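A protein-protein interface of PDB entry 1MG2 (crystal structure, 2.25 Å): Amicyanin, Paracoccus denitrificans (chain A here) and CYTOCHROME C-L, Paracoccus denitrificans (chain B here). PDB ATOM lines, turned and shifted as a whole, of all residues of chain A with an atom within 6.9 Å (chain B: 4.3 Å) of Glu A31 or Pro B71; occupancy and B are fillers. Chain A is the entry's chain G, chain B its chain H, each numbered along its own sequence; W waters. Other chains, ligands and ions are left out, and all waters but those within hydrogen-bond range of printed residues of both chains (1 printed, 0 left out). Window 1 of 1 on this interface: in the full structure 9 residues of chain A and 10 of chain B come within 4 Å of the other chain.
Printed residues of chain B within 4 Å of Glu A31: Gly B67, Gly B70, Pro B71, Gly B72 and Asp B75. Of the printed residues of chain A, Pro B71 touches Glu A31 and Thr A32. Of the printed residues of chain A, Gly B67 touches Glu A31 (3.7 Å) and Pro A33 (3.5 Å). Of the printed residues of chain A, Gly B72 touches Glu A31 (2.8 Å). Printed residues of chain A within 4 Å of Asp B75: Lys A27 (3.9 Å), Lys A29 (2.9 Å) and Glu A31 (2.5 Å). Of the printed residues of chain A, Gly B70 touches Glu A31. Of the printed residues of chain B, Lys A27 touches Asp B75 (3.9 Å). Tyr A30 touches none of the printed residues of chain B. The nearest residue of chain A that does not touch Pro B71 is Pro A33 (5.8 Å). The nearest printed residue of chain B that does not touch Lys A27 is Glu B66 (8.8 Å).
Hydrophobic or aromatic side chains of chain B within 4 Å of the printed part of chain A: Pro B71. Among the printed residues, Asp or Glu carboxylates within 4 Å of a Lys or Arg side-chain nitrogen of the other chain: Lys A29 with Asp B75 (2.9 Å).
The backbone NH (N) of Glu A31 sits at hydrogen-bond distance from the backbone carbonyl oxygen (O) of Asp A24. The backbone carbonyl oxygen (O) of His B61 is in hydrogen-bond range of the backbone NH (N) of Gly B67. A ring nitrogen (ND1) of His B61 sits at hydrogen-bond distance from the backbone carbonyl oxygen (O) of Pro B71, at 2.6 Å.
The side-chain amino group (NZ) of Lys A29 lies within salt-bridge range of the side-chain carboxylate (OD1) of Asp B75 (2.9 Å). The backbone carbonyl oxygen (O) of Glu A31 is in hydrogen-bond range of the backbone NH (N) of Gly B72 (2.8 Å). OE1 of Glu A31 lies close to OD1 of Asp B75 (2.5 Å).
Water W1 bridges O of Tyr A30 (2.6 Å) and O of Glu B66 (3.0 Å).
CG of Lys A27 touches OD1 of Asp B75 (3.9 Å). O of Glu A31 touches CA of Gly B67 (3.7 Å). O of Gly B70 touches O of Glu A31 (3.998 Å). Glu A31 touches Pro B71. CA of Pro B71 touches OG1 of Thr A32, 3.4 Å away. C of Gly B67 touches CD of Pro A33, 3.5 Å away.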
ATOM      1  N   VAL A  22     -15.565 -16.006   7.283  1.00  0.00           N
ATOM      2  CA  VAL A  22     -15.937 -14.719   7.848  1.00  0.00           C
ATOM      3  C   VAL A  22     -17.424 -14.409   7.792  1.00  0.00           C
ATOM      4  O   VAL A  22     -18.111 -14.732   6.824  1.00  0.00           O
ATOM      5  CB  VAL A  22     -15.178 -13.562   7.139  1.00  0.00           C
ATOM      6  CG1 VAL A  22     -15.669 -12.219   7.651  1.00  0.00           C
ATOM      7  CG2 VAL A  22     -13.682 -13.685   7.386  1.00  0.00           C
ATOM      8  N   VAL A  23     -17.908 -13.797   8.863  1.00  0.00           N
ATOM      9  CA  VAL A  23     -19.285 -13.357   8.959  1.00  0.00           C
ATOM     10  C   VAL A  23     -19.165 -11.853   9.189  1.00  0.00           C
ATOM     11  O   VAL A  23     -18.727 -11.426  10.256  1.00  0.00           O
ATOM     12  CB  VAL A  23     -20.019 -13.964  10.170  1.00  0.00           C
ATOM     13  CG1 VAL A  23     -21.401 -13.330  10.293  1.00  0.00           C
ATOM     14  CG2 VAL A  23     -20.150 -15.475  10.008  1.00  0.00           C
ATOM     15  N   ASP A  24     -19.513 -11.052   8.186  1.00  0.00           N
ATOM     16  CA  ASP A  24     -19.438  -9.601   8.331  1.00  0.00           C
ATOM     17  C   ASP A  24     -20.689  -9.056   9.003  1.00  0.00           C
ATOM     18  O   ASP A  24     -21.792  -9.559   8.796  1.00  0.00           O
ATOM     19  CB  ASP A  24     -19.276  -8.925   6.968  1.00  0.00           C
ATOM     20  CG  ASP A  24     -17.897  -9.104   6.397  1.00  0.00           C
ATOM     21  OD1 ASP A  24     -16.922  -8.630   7.020  1.00  0.00           O
ATOM     22  OD2 ASP A  24     -17.782  -9.720   5.322  1.00  0.00           O
ATOM     23  N   ILE A  25     -20.509  -8.024   9.815  1.00  0.00           N
ATOM     24  CA  ILE A  25     -21.621  -7.398  10.507  1.00  0.00           C
ATOM     25  C   ILE A  25     -21.743  -5.964   9.999  1.00  0.00           C
ATOM     26  O   ILE A  25     -20.776  -5.198  10.041  1.00  0.00           O
ATOM     27  CB  ILE A  25     -21.383  -7.362  12.022  1.00  0.00           C
ATOM     28  CG1 ILE A  25     -20.991  -8.751  12.523  1.00  0.00           C
ATOM     29  CG2 ILE A  25     -22.644  -6.898  12.729  1.00  0.00           C
ATOM     30  CD1 ILE A  25     -20.487  -8.772  13.957  1.00  0.00           C
ATOM     31  N   ALA A  26     -22.922  -5.607   9.501  1.00  0.00           N
ATOM     32  CA  ALA A  26     -23.142  -4.259   8.996  1.00  0.00           C
ATOM     33  C   ALA A  26     -24.629  -3.999   8.864  1.00  0.00           C
ATOM     34  O   ALA A  26     -25.419  -4.933   8.743  1.00  0.00           O
ATOM     35  CB  ALA A  26     -22.453  -4.085   7.647  1.00  0.00           C
ATOM     36  N   LYS A  27     -25.010  -2.729   8.898  1.00  0.00           N
ATOM     37  CA  LYS A  27     -26.412  -2.362   8.785  1.00  0.00           C
ATOM     38  C   LYS A  27     -27.302  -3.117   9.772  1.00  0.00           C
ATOM     39  O   LYS A  27     -28.390  -3.572   9.422  1.00  0.00           O
ATOM     40  CB  LYS A  27     -26.899  -2.608   7.356  1.00  0.00           C
ATOM     41  CG  LYS A  27     -26.356  -1.617   6.355  1.00  0.00           C
ATOM     42  CD  LYS A  27     -26.831  -0.217   6.701  1.00  0.00           C
ATOM     43  CE  LYS A  27     -26.246   0.810   5.761  1.00  0.00           C
ATOM     44  NZ  LYS A  27     -24.762   0.776   5.801  1.00  0.00           N
ATOM     45  N   MET A  28     -26.831  -3.254  11.004  1.00  0.00           N
ATOM     46  CA  MET A  28     -27.599  -3.929  12.041  1.00  0.00           C
ATOM     47  C   MET A  28     -27.921  -5.380  11.725  1.00  0.00           C
ATOM     48  O   MET A  28     -29.005  -5.868  12.048  1.00  0.00           O
ATOM     49  CB  MET A  28     -28.905  -3.174  12.302  1.00  0.00           C
ATOM     50  CG  MET A  28     -28.707  -1.717  12.695  1.00  0.00           C
ATOM     51  SD  MET A  28     -27.537  -1.537  14.049  1.00  0.00           S
ATOM     52  CE  MET A  28     -28.584  -1.933  15.443  1.00  0.00           C
ATOM     53  N   LYS A  29     -26.988  -6.080  11.098  1.00  0.00           N
ATOM     54  CA  LYS A  29     -27.245  -7.472  10.792  1.00  0.00           C
ATOM     55  C   LYS A  29     -25.980  -8.268  10.530  1.00  0.00           C
ATOM     56  O   LYS A  29     -24.922  -7.715  10.221  1.00  0.00           O
ATOM     57  CB  LYS A  29     -28.171  -7.596   9.572  1.00  0.00           C
ATOM     58  CG  LYS A  29     -27.494  -7.366   8.226  1.00  0.00           C
ATOM     59  CD  LYS A  29     -28.402  -7.793   7.069  1.00  0.00           C
ATOM     60  CE  LYS A  29     -29.188  -6.627   6.476  1.00  0.00           C
ATOM     61  NZ  LYS A  29     -28.333  -5.778   5.592  1.00  0.00           N
ATOM     62  N   TYR A  30     -26.097  -9.579  10.686  1.00  0.00           N
ATOM     63  CA  TYR A  30     -24.993 -10.474  10.401  1.00  0.00           C
ATOM     64  C   TYR A  30     -25.213 -10.775   8.922  1.00  0.00           C
ATOM     65  O   TYR A  30     -26.217 -11.383   8.563  1.00  0.00           O
ATOM     66  CB  TYR A  30     -25.115 -11.750  11.232  1.00  0.00           C
ATOM     67  CG  TYR A  30     -24.980 -11.521  12.718  1.00  0.00           C
ATOM     68  CD1 TYR A  30     -23.760 -11.129  13.276  1.00  0.00           C
ATOM     69  CD2 TYR A  30     -26.070 -11.689  13.568  1.00  0.00           C
ATOM     70  CE1 TYR A  30     -23.628 -10.912  14.651  1.00  0.00           C
ATOM     71  CE2 TYR A  30     -25.952 -11.476  14.941  1.00  0.00           C
ATOM     72  CZ  TYR A  30     -24.728 -11.088  15.476  1.00  0.00           C
ATOM     73  OH  TYR A  30     -24.609 -10.892  16.832  1.00  0.00           O
ATOM     74  N   GLU A  31     -24.295 -10.331   8.069  1.00  0.00           N
ATOM     75  CA  GLU A  31     -24.432 -10.535   6.629  1.00  0.00           C
ATOM     76  C   GLU A  31     -24.683 -11.985   6.206  1.00  0.00           C
ATOM     77  O   GLU A  31     -25.322 -12.226   5.184  1.00  0.00           O
ATOM     78  CB  GLU A  31     -23.207  -9.972   5.901  1.00  0.00           C
ATOM     79  CG  GLU A  31     -23.062  -8.447   6.019  1.00  0.00           C
ATOM     80  CD  GLU A  31     -24.148  -7.662   5.280  1.00  0.00           C
ATOM     81  OE1 GLU A  31     -24.233  -6.430   5.485  1.00  0.00           O
ATOM     82  OE2 GLU A  31     -24.915  -8.258   4.491  1.00  0.00           O
ATOM     83  N   THR A  32     -24.178 -12.940   6.983  1.00  0.00           N
ATOM     84  CA  THR A  32     -24.375 -14.367   6.697  1.00  0.00           C
ATOM     85  C   THR A  32     -25.055 -15.012   7.907  1.00  0.00           C
ATOM     86  O   THR A  32     -24.392 -15.605   8.754  1.00  0.00           O
ATOM     87  CB  THR A  32     -23.032 -15.082   6.440  1.00  0.00           C
ATOM     88  OG1 THR A  32     -22.366 -14.474   5.326  1.00  0.00           O
ATOM     89  CG2 THR A  32     -23.268 -16.554   6.131  1.00  0.00           C
ATOM     90  N   PRO A  33     -26.392 -14.921   7.988  1.00  0.00           N
ATOM     91  CA  PRO A  33     -27.213 -15.464   9.079  1.00  0.00           C
ATOM     92  C   PRO A  33     -27.091 -16.960   9.337  1.00  0.00           C
ATOM     93  O   PRO A  33     -27.109 -17.399  10.480  1.00  0.00           O
ATOM     94  CB  PRO A  33     -28.647 -15.101   8.665  1.00  0.00           C
ATOM     95  CG  PRO A  33     -28.485 -14.043   7.622  1.00  0.00           C
ATOM     96  CD  PRO A  33     -27.251 -14.458   6.887  1.00  0.00           C
ATOM     97  N   GLU A  34     -26.982 -17.743   8.274  1.00  0.00           N
ATOM     98  CA  GLU A  34     -26.908 -19.189   8.417  1.00  0.00           C
ATOM     99  C   GLU A  34     -25.615 -19.774   7.863  1.00  0.00           C
ATOM    100  O   GLU A  34     -25.613 -20.403   6.809  1.00  0.00           O
ATOM    101  CB  GLU A  34     -28.105 -19.813   7.711  1.00  0.00           C
ATOM    102  CG  GLU A  34     -28.391 -21.242   8.107  1.00  0.00           C
ATOM    103  CD  GLU A  34     -29.433 -21.881   7.206  1.00  0.00           C
ATOM    104  OE1 GLU A  34     -30.519 -21.277   7.040  1.00  0.00           O
ATOM    105  OE2 GLU A  34     -29.161 -22.980   6.666  1.00  0.00           O
ATOM    106  N   ARG A  48     -18.240  -4.145  10.576  1.00  0.00           N
ATOM    107  CA  ARG A  48     -17.864  -3.201   9.530  1.00  0.00           C
ATOM    108  C   ARG A  48     -18.410  -1.787   9.718  1.00  0.00           C
ATOM    109  O   ARG A  48     -18.096  -0.891   8.929  1.00  0.00           O
ATOM    110  CB  ARG A  48     -18.313  -3.735   8.170  1.00  0.00           C
ATOM    111  CG  ARG A  48     -17.717  -5.091   7.791  1.00  0.00           C
ATOM    112  CD  ARG A  48     -16.197  -5.035   7.739  1.00  0.00           C
ATOM    113  NE  ARG A  48     -15.628  -6.270   7.216  1.00  0.00           N
ATOM    114  CZ  ARG A  48     -14.333  -6.466   6.985  1.00  0.00           C
ATOM    115  NH1 ARG A  48     -13.919  -7.629   6.503  1.00  0.00           N
ATOM    116  NH2 ARG A  48     -13.452  -5.503   7.238  1.00  0.00           N
ATOM    117  N   HIS B  61     -28.540 -17.106  -0.956  1.00  0.00           N
ATOM    118  CA  HIS B  61     -28.511 -15.699  -0.561  1.00  0.00           C
ATOM    119  C   HIS B  61     -29.795 -15.097  -0.001  1.00  0.00           C
ATOM    120  O   HIS B  61     -29.816 -13.918   0.374  1.00  0.00           O
ATOM    121  CB  HIS B  61     -28.021 -14.855  -1.736  1.00  0.00           C
ATOM    122  CG  HIS B  61     -26.551 -14.980  -1.994  1.00  0.00           C
ATOM    123  ND1 HIS B  61     -25.639 -14.411  -1.150  1.00  0.00           N
ATOM    124  CD2 HIS B  61     -26.130 -15.663  -3.075  1.00  0.00           C
ATOM    125  CE1 HIS B  61     -24.460 -14.766  -1.771  1.00  0.00           C
ATOM    126  NE2 HIS B  61     -24.739 -15.532  -2.950  1.00  0.00           N
ATOM    127  N   GLU B  66     -30.988 -10.728   1.328  1.00  0.00           N
ATOM    128  CA  GLU B  66     -30.673 -10.170   2.641  1.00  0.00           C
ATOM    129  C   GLU B  66     -29.576 -11.031   3.267  1.00  0.00           C
ATOM    130  O   GLU B  66     -28.948 -10.644   4.250  1.00  0.00           O
ATOM    131  CB  GLU B  66     -31.905 -10.182   3.556  1.00  0.00           C
ATOM    132  CG  GLU B  66     -32.287 -11.567   4.084  1.00  0.00           C
ATOM    133  CD  GLU B  66     -33.245 -12.319   3.172  1.00  0.00           C
ATOM    134  OE1 GLU B  66     -33.248 -12.058   1.948  1.00  0.00           O
ATOM    135  OE2 GLU B  66     -33.992 -13.187   3.682  1.00  0.00           O
ATOM    136  N   GLY B  67     -29.359 -12.206   2.687  1.00  0.00           N
ATOM    137  CA  GLY B  67     -28.335 -13.101   3.192  1.00  0.00           C
ATOM    138  C   GLY B  67     -28.905 -14.356   3.808  1.00  0.00           C
ATOM    139  O   GLY B  67     -30.030 -14.354   4.302  1.00  0.00           O
ATOM    140  N   GLY B  70     -25.135 -17.727   2.031  1.00  0.00           N
ATOM    141  CA  GLY B  70     -24.157 -16.821   1.466  1.00  0.00           C
ATOM    142  C   GLY B  70     -24.444 -15.445   2.033  1.00  0.00           C
ATOM    143  O   GLY B  70     -25.548 -15.204   2.526  1.00  0.00           O
ATOM    144  N   PRO B  71     -23.482 -14.518   1.980  1.00  0.00           N
ATOM    145  CA  PRO B  71     -23.663 -13.164   2.507  1.00  0.00           C
ATOM    146  C   PRO B  71     -24.755 -12.371   1.798  1.00  0.00           C
ATOM    147  O   PRO B  71     -25.083 -12.646   0.649  1.00  0.00           O
ATOM    148  CB  PRO B  71     -22.285 -12.541   2.319  1.00  0.00           C
ATOM    149  CG  PRO B  71     -21.812 -13.201   1.055  1.00  0.00           C
ATOM    150  CD  PRO B  71     -22.176 -14.646   1.318  1.00  0.00           C
ATOM    151  N   GLY B  72     -25.324 -11.392   2.493  1.00  0.00           N
ATOM    152  CA  GLY B  72     -26.352 -10.576   1.878  1.00  0.00           C
ATOM    153  C   GLY B  72     -25.763  -9.804   0.711  1.00  0.00           C
ATOM    154  O   GLY B  72     -24.569  -9.516   0.677  1.00  0.00           O
ATOM    155  N   LEU B  73     -26.608  -9.462  -0.250  1.00  0.00           N
ATOM    156  CA  LEU B  73     -26.176  -8.729  -1.431  1.00  0.00           C
ATOM    157  C   LEU B  73     -26.941  -7.403  -1.557  1.00  0.00           C
ATOM    158  O   LEU B  73     -26.742  -6.659  -2.517  1.00  0.00           O
ATOM    159  CB  LEU B  73     -26.446  -9.580  -2.677  1.00  0.00           C
ATOM    160  CG  LEU B  73     -25.523 -10.709  -3.156  1.00  0.00           C
ATOM    161  CD1 LEU B  73     -24.714 -11.311  -2.035  1.00  0.00           C
ATOM    162  CD2 LEU B  73     -26.388 -11.764  -3.840  1.00  0.00           C
ATOM    163  N   ASP B  75     -26.956  -4.519   0.489  1.00  0.00           N
ATOM    164  CA  ASP B  75     -26.543  -3.293   1.161  1.00  0.00           C
ATOM    165  C   ASP B  75     -25.180  -2.762   0.727  1.00  0.00           C
ATOM    166  O   ASP B  75     -24.522  -3.331  -0.148  1.00  0.00           O
ATOM    167  CB  ASP B  75     -26.608  -3.455   2.688  1.00  0.00           C
ATOM    168  CG  ASP B  75     -25.645  -4.493   3.220  1.00  0.00           C
ATOM    169  OD1 ASP B  75     -25.832  -4.901   4.385  1.00  0.00           O
ATOM    170  OD2 ASP B  75     -24.708  -4.892   2.495  1.00  0.00           O
HETATM  171  O   HOH W   1     -28.395 -11.143   7.194  1.00  0.00           O
